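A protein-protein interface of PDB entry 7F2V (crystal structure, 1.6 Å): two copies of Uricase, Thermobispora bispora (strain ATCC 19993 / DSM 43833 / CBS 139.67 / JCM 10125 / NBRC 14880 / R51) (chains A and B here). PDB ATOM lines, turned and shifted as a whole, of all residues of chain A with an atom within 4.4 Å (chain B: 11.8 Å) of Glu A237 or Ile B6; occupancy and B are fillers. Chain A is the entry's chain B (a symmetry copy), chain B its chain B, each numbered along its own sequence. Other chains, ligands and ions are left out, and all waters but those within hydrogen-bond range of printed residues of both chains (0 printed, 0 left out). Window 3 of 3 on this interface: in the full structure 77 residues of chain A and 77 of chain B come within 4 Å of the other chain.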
ATOM      1  N   TYR A 229      24.871   5.339  -6.041  1.00  0.00           N
ATOM      2  CA  TYR A 229      25.349   4.676  -7.250  1.00  0.00           C
ATOM      3  C   TYR A 229      26.410   3.626  -6.926  1.00  0.00           C
ATOM      4  O   TYR A 229      26.414   2.532  -7.505  1.00  0.00           O
ATOM      5  CB  TYR A 229      25.906   5.696  -8.248  1.00  0.00           C
ATOM      6  CG  TYR A 229      26.253   5.028  -9.552  1.00  0.00           C
ATOM      7  CD1 TYR A 229      25.269   4.744 -10.483  1.00  0.00           C
ATOM      8  CD2 TYR A 229      27.548   4.618  -9.823  1.00  0.00           C
ATOM      9  CE1 TYR A 229      25.572   4.102 -11.661  1.00  0.00           C
ATOM     10  CE2 TYR A 229      27.853   3.969 -11.005  1.00  0.00           C
ATOM     11  CZ  TYR A 229      26.856   3.723 -11.915  1.00  0.00           C
ATOM     12  OH  TYR A 229      27.141   3.079 -13.093  1.00  0.00           O
ATOM     13  N   SER A 233      25.701  -0.220  -7.858  1.00  0.00           N
ATOM     14  CA  SER A 233      26.525  -0.883  -8.861  1.00  0.00           C
ATOM     15  C   SER A 233      27.299  -2.049  -8.257  1.00  0.00           C
ATOM     16  O   SER A 233      27.479  -3.081  -8.916  1.00  0.00           O
ATOM     17  CB  SER A 233      27.463   0.121  -9.534  1.00  0.00           C
ATOM     18  OG  SER A 233      28.275   0.769  -8.592  1.00  0.00           O
ATOM     19  N   ALA A 234      27.749  -1.917  -7.002  1.00  0.00           N
ATOM     20  CA  ALA A 234      28.403  -3.038  -6.333  1.00  0.00           C
ATOM     21  C   ALA A 234      27.481  -4.243  -6.255  1.00  0.00           C
ATOM     22  O   ALA A 234      27.925  -5.380  -6.448  1.00  0.00           O
ATOM     23  CB  ALA A 234      28.857  -2.633  -4.929  1.00  0.00           C
ATOM     24  N   VAL A 235      26.197  -4.016  -5.958  1.00  0.00           N
ATOM     25  CA  VAL A 235      25.223  -5.109  -5.918  1.00  0.00           C
ATOM     26  C   VAL A 235      25.123  -5.794  -7.284  1.00  0.00           C
ATOM     27  O   VAL A 235      25.184  -7.026  -7.389  1.00  0.00           O
ATOM     28  CB  VAL A 235      23.853  -4.587  -5.440  1.00  0.00           C
ATOM     29  CG1 VAL A 235      22.769  -5.621  -5.692  1.00  0.00           C
ATOM     30  CG2 VAL A 235      23.916  -4.246  -3.954  1.00  0.00           C
ATOM     31  N   LEU A 236      24.971  -5.009  -8.353  1.00  0.00           N
ATOM     32  CA  LEU A 236      24.843  -5.594  -9.688  1.00  0.00           C
ATOM     33  C   LEU A 236      26.104  -6.362 -10.097  1.00  0.00           C
ATOM     34  O   LEU A 236      26.017  -7.443 -10.691  1.00  0.00           O
ATOM     35  CB  LEU A 236      24.523  -4.498 -10.704  1.00  0.00           C
ATOM     36  CG  LEU A 236      23.187  -3.770 -10.519  1.00  0.00           C
ATOM     37  CD1 LEU A 236      22.850  -2.952 -11.744  1.00  0.00           C
ATOM     38  CD2 LEU A 236      22.062  -4.758 -10.206  1.00  0.00           C
ATOM     39  N   GLU A 237      27.285  -5.823  -9.782  1.00  0.00           N
ATOM     40  CA  GLU A 237      28.530  -6.512 -10.117  1.00  0.00           C
ATOM     41  C   GLU A 237      28.632  -7.866  -9.428  1.00  0.00           C
ATOM     42  O   GLU A 237      29.117  -8.841 -10.020  1.00  0.00           O
ATOM     43  CB  GLU A 237      29.730  -5.649  -9.733  1.00  0.00           C
ATOM     44  CG  GLU A 237      30.063  -4.571 -10.725  1.00  0.00           C
ATOM     45  CD  GLU A 237      30.822  -3.414 -10.068  1.00  0.00           C
ATOM     46  OE1 GLU A 237      32.028  -3.561  -9.827  1.00  0.00           O
ATOM     47  OE2 GLU A 237      30.181  -2.387  -9.804  1.00  0.00           O
ATOM     48  N   ALA A 238      28.227  -7.938  -8.164  1.00  0.00           N
ATOM     49  CA  ALA A 238      28.351  -9.179  -7.414  1.00  0.00           C
ATOM     50  C   ALA A 238      27.232 -10.159  -7.719  1.00  0.00           C
ATOM     51  O   ALA A 238      27.386 -11.350  -7.437  1.00  0.00           O
ATOM     52  CB  ALA A 238      28.373  -8.905  -5.910  1.00  0.00           C
ATOM     53  N   HIS A 239      26.123  -9.693  -8.299  1.00  0.00           N
ATOM     54  CA  HIS A 239      24.923 -10.505  -8.494  1.00  0.00           C
ATOM     55  C   HIS A 239      24.401 -10.337  -9.913  1.00  0.00           C
ATOM     56  O   HIS A 239      23.500  -9.526 -10.173  1.00  0.00           O
ATOM     57  CB  HIS A 239      23.861 -10.141  -7.461  1.00  0.00           C
ATOM     58  CG  HIS A 239      24.235 -10.566  -6.079  1.00  0.00           C
ATOM     59  ND1 HIS A 239      24.112 -11.868  -5.653  1.00  0.00           N
ATOM     60  CD2 HIS A 239      24.801  -9.883  -5.055  1.00  0.00           C
ATOM     61  CE1 HIS A 239      24.555 -11.967  -4.412  1.00  0.00           C
ATOM     62  NE2 HIS A 239      24.979 -10.776  -4.026  1.00  0.00           N
ATOM     63  N   VAL A 285      20.036   1.885 -10.607  1.00  0.00           N
ATOM     64  CA  VAL A 285      21.218   1.321 -11.254  1.00  0.00           C
ATOM     65  C   VAL A 285      20.760   0.089 -12.016  1.00  0.00           C
ATOM     66  O   VAL A 285      20.070  -0.771 -11.455  1.00  0.00           O
ATOM     67  CB  VAL A 285      22.321   0.981 -10.233  1.00  0.00           C
ATOM     68  CG1 VAL A 285      23.613   0.561 -10.958  1.00  0.00           C
ATOM     69  CG2 VAL A 285      22.560   2.181  -9.331  1.00  0.00           C
ATOM     70  N   VAL A 286      21.091   0.026 -13.309  1.00  0.00           N
ATOM     71  CA  VAL A 286      20.462  -0.950 -14.190  1.00  0.00           C
ATOM     72  C   VAL A 286      21.503  -1.634 -15.059  1.00  0.00           C
ATOM     73  O   VAL A 286      22.542  -1.060 -15.401  1.00  0.00           O
ATOM     74  CB  VAL A 286      19.370  -0.306 -15.075  1.00  0.00           C
ATOM     75  CG1 VAL A 286      18.379   0.442 -14.224  1.00  0.00           C
ATOM     76  CG2 VAL A 286      19.973   0.634 -16.096  1.00  0.00           C
ATOM     77  N   ARG A 287      21.209  -2.885 -15.404  1.00  0.00           N
ATOM     78  CA  ARG A 287      21.937  -3.612 -16.438  1.00  0.00           C
ATOM     79  C   ARG A 287      21.402  -3.164 -17.793  1.00  0.00           C
ATOM     80  O   ARG A 287      20.244  -3.424 -18.128  1.00  0.00           O
ATOM     81  CB  ARG A 287      21.774  -5.117 -16.248  1.00  0.00           C
ATOM     82  CG  ARG A 287      22.532  -5.680 -15.050  1.00  0.00           C
ATOM     83  CD  ARG A 287      23.913  -6.137 -15.467  1.00  0.00           C
ATOM     84  NE  ARG A 287      23.809  -7.168 -16.496  1.00  0.00           N
ATOM     85  CZ  ARG A 287      23.555  -8.448 -16.243  1.00  0.00           C
ATOM     86  NH1 ARG A 287      23.406  -8.859 -14.988  1.00  0.00           N
ATOM     87  NH2 ARG A 287      23.452  -9.319 -17.240  1.00  0.00           N
ATOM     88  N   ALA B   5      28.095  -2.729 -18.972  1.00  0.00           N
ATOM     89  CA  ALA B   5      26.702  -3.141 -18.930  1.00  0.00           C
ATOM     90  C   ALA B   5      25.925  -2.399 -17.825  1.00  0.00           C
ATOM     91  O   ALA B   5      24.727  -2.171 -17.953  1.00  0.00           O
ATOM     92  CB  ALA B   5      26.608  -4.649 -18.729  1.00  0.00           C
ATOM     93  N   ILE B   6      26.615  -2.000 -16.761  1.00  0.00           N
ATOM     94  CA  ILE B   6      25.967  -1.389 -15.604  1.00  0.00           C
ATOM     95  C   ILE B   6      25.996   0.128 -15.762  1.00  0.00           C
ATOM     96  O   ILE B   6      27.069   0.721 -15.925  1.00  0.00           O
ATOM     97  CB  ILE B   6      26.660  -1.820 -14.306  1.00  0.00           C
ATOM     98  CG1 ILE B   6      26.429  -3.311 -14.062  1.00  0.00           C
ATOM     99  CG2 ILE B   6      26.205  -0.950 -13.141  1.00  0.00           C
ATOM    100  CD1 ILE B   6      27.399  -3.904 -13.049  1.00  0.00           C
ATOM    101  N   VAL B   7      24.822   0.760 -15.697  1.00  0.00           N
ATOM    102  CA  VAL B   7      24.694   2.197 -15.908  1.00  0.00           C
ATOM    103  C   VAL B   7      23.695   2.792 -14.920  1.00  0.00           C
ATOM    104  O   VAL B   7      22.889   2.094 -14.296  1.00  0.00           O
ATOM    105  CB  VAL B   7      24.242   2.549 -17.348  1.00  0.00           C
ATOM    106  CG1 VAL B   7      25.260   2.072 -18.382  1.00  0.00           C
ATOM    107  CG2 VAL B   7      22.868   1.968 -17.636  1.00  0.00           C
ATOM    108  N   LEU B   8      23.744   4.114 -14.812  1.00  0.00           N
ATOM    109  CA  LEU B   8      22.720   4.850 -14.089  1.00  0.00           C
ATOM    110  C   LEU B   8      21.430   4.869 -14.901  1.00  0.00           C
ATOM    111  O   LEU B   8      21.448   5.099 -16.118  1.00  0.00           O
ATOM    112  CB  LEU B   8      23.209   6.271 -13.805  1.00  0.00           C
ATOM    113  CG  LEU B   8      22.274   7.204 -13.022  1.00  0.00           C
ATOM    114  CD1 LEU B   8      22.180   6.789 -11.566  1.00  0.00           C
ATOM    115  CD2 LEU B   8      22.726   8.652 -13.138  1.00  0.00           C
ATOM    116  N   GLY B   9      20.316   4.602 -14.239  1.00  0.00           N
ATOM    117  CA  GLY B   9      19.009   4.659 -14.868  1.00  0.00           C
ATOM    118  C   GLY B   9      18.263   5.914 -14.470  1.00  0.00           C
ATOM    119  O   GLY B   9      18.860   6.991 -14.327  1.00  0.00           O
ATOM    120  N   ARG B  10      16.947   5.771 -14.295  1.00  0.00           N
ATOM    121  CA  ARG B  10      16.123   6.878 -13.841  1.00  0.00           C
ATOM    122  C   ARG B  10      16.625   7.376 -12.490  1.00  0.00           C
ATOM    123  O   ARG B  10      17.123   6.605 -11.669  1.00  0.00           O
ATOM    124  CB  ARG B  10      14.664   6.433 -13.724  1.00  0.00           C
ATOM    125  CG  ARG B  10      14.446   5.319 -12.702  1.00  0.00           C
ATOM    126  CD  ARG B  10      12.964   5.061 -12.468  1.00  0.00           C
ATOM    127  NE  ARG B  10      12.347   4.366 -13.594  1.00  0.00           N
ATOM    128  CZ  ARG B  10      11.040   4.136 -13.699  1.00  0.00           C
ATOM    129  NH1 ARG B  10      10.216   4.556 -12.745  1.00  0.00           N
ATOM    130  NH2 ARG B  10      10.560   3.491 -14.760  1.00  0.00           N
ATOM    131  N   THR B  46      24.191  12.598 -14.267  1.00  0.00           N
ATOM    132  CA  THR B  46      24.898  11.327 -14.340  1.00  0.00           C
ATOM    133  C   THR B  46      26.252  11.410 -13.650  1.00  0.00           C
ATOM    134  O   THR B  46      26.598  10.543 -12.842  1.00  0.00           O
ATOM    135  CB  THR B  46      25.049  10.915 -15.803  1.00  0.00           C
ATOM    136  OG1 THR B  46      23.745  10.818 -16.395  1.00  0.00           O
ATOM    137  CG2 THR B  46      25.745   9.563 -15.916  1.00  0.00           C
ATOM    138  N   HIS B  49      26.398  11.210  -9.886  1.00  0.00           N
ATOM    139  CA  HIS B  49      26.284   9.848  -9.383  1.00  0.00           C
ATOM    140  C   HIS B  49      27.540   9.032  -9.651  1.00  0.00           C
ATOM    141  O   HIS B  49      28.035   8.339  -8.758  1.00  0.00           O
ATOM    142  CB  HIS B  49      25.098   9.132 -10.036  1.00  0.00           C
ATOM    143  CG  HIS B  49      23.761   9.643  -9.606  1.00  0.00           C
ATOM    144  ND1 HIS B  49      23.206  10.801 -10.106  1.00  0.00           N
ATOM    145  CD2 HIS B  49      22.849   9.128  -8.748  1.00  0.00           C
ATOM    146  CE1 HIS B  49      22.014  10.985  -9.564  1.00  0.00           C
ATOM    147  NE2 HIS B  49      21.772   9.980  -8.739  1.00  0.00           N
ATOM    148  N   VAL B  50      28.054   9.094 -10.879  1.00  0.00           N
ATOM    149  CA  VAL B  50      29.071   8.133 -11.299  1.00  0.00           C
ATOM    150  C   VAL B  50      30.467   8.553 -10.858  1.00  0.00           C
ATOM    151  O   VAL B  50      31.245   7.725 -10.378  1.00  0.00           O
ATOM    152  CB  VAL B  50      29.008   7.924 -12.821  1.00  0.00           C
ATOM    153  CG1 VAL B  50      30.135   7.007 -13.258  1.00  0.00           C
ATOM    154  CG2 VAL B  50      27.664   7.343 -13.208  1.00  0.00           C
ATOM    155  N   THR B  51      30.803   9.831 -11.009  1.00  0.00           N
ATOM    156  CA  THR B  51      32.131  10.310 -10.654  1.00  0.00           C
ATOM    157  C   THR B  51      32.158  11.163  -9.395  1.00  0.00           C
ATOM    158  O   THR B  51      33.238  11.348  -8.825  1.00  0.00           O
ATOM    159  CB  THR B  51      32.745  11.121 -11.808  1.00  0.00           C
ATOM    160  OG1 THR B  51      32.123  12.409 -11.889  1.00  0.00           O
ATOM    161  CG2 THR B  51      32.575  10.394 -13.138  1.00  0.00           C
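Among the printed residues, pairs that only touch across the chains: Tyr A229 with Ile B6 (3.7 Å), Tyr A229 with Val B7 (3.8 Å), Tyr A229 with Leu B8 (3.6 Å), Tyr A229 with His B49 (3.4 Å), Tyr A229 with Val B50 (3.9 Å), Ser A233 with Ile B6 (3.97 Å), Leu A236 with Ile B6 (3.8 Å), Glu A237 with Ile B6 (3.6 Å), Val A285 with Ile B6 (3.7 Å), Val A285 with Val B7 (3.6 Å), Val A286 with Ala B5 (3.5 Å), Val A286 with Ile B6 (3.4 Å) and Arg A287 with Ala B5 (3.5 Å).
Of the 10 printed residues of chain B, 6 touch a printed residue of chain A.
Printed residues of chain A that touch a printed residue of chain B: Tyr A229, Ser A233, Leu A236, Glu A237, Val A285, Val A286 and Arg A287.
Hydrophobic or aromatic side chains of chain A that line the printed part of chain B: Tyr A229, Leu A236, Val A285 and Val A286.
Along chain A the printed residues that touch a printed residue of chain B span positions 229 to 287.
Among the printed residues, 14 pairs touch across the chains.
Among the printed residues, no Asp or Glu carboxylate lies within 4 Å of a Lys or Arg side-chain nitrogen of the other chain.
No position is printed for both chains.
Of the 14 pairs that touch across the chains among the printed residues, none has its exchanged pair printed and touching as well.
The side-chain hydroxyl of Ser A233 lies within hydrogen-bond range of the backbone carbonyl oxygen of Tyr A229.
Ser A233 touches just one residue of chain B: Ile B6 (3.97 Å).
No residue of chain B comes within 4 Å of Ala A234.
No residue of chain B comes within 4 Å of Val A235.
Of chain B, only Ile B6 (3.8 Å) comes within 4 Å of Leu A236.
Of the printed residues of chain B, Glu A237 touches Ile B6.
No residue of chain B comes within 4 Å of Ala A238.
Of chain B, only Ile B6 and Val B7 come within 4 Å of Val A285.
Of the printed residues of chain B, Val A286 touches Ala B5, Ile B6 and Val B7.
Arg A287 touches just one residue of chain B: Ala B5 (3.5 Å).
Ile B6 touches six residues of chain A.
Printed residues of chain A within 4 Å of Val B7: Tyr A229, Val A285 and Val A286.
Of the printed residues of chain A, Val B50 touches Tyr A229.
The nearest residue of chain B that does not touch Glu A237 is Ala B5 (8.5 Å).
The nearest printed residue of chain B that does not touch Tyr A229 is Gly B9 (5.9 Å).
The backbone carbonyl oxygen of Val B7 is in hydrogen-bond range of the backbone NH of Val A286 (2.9 Å).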
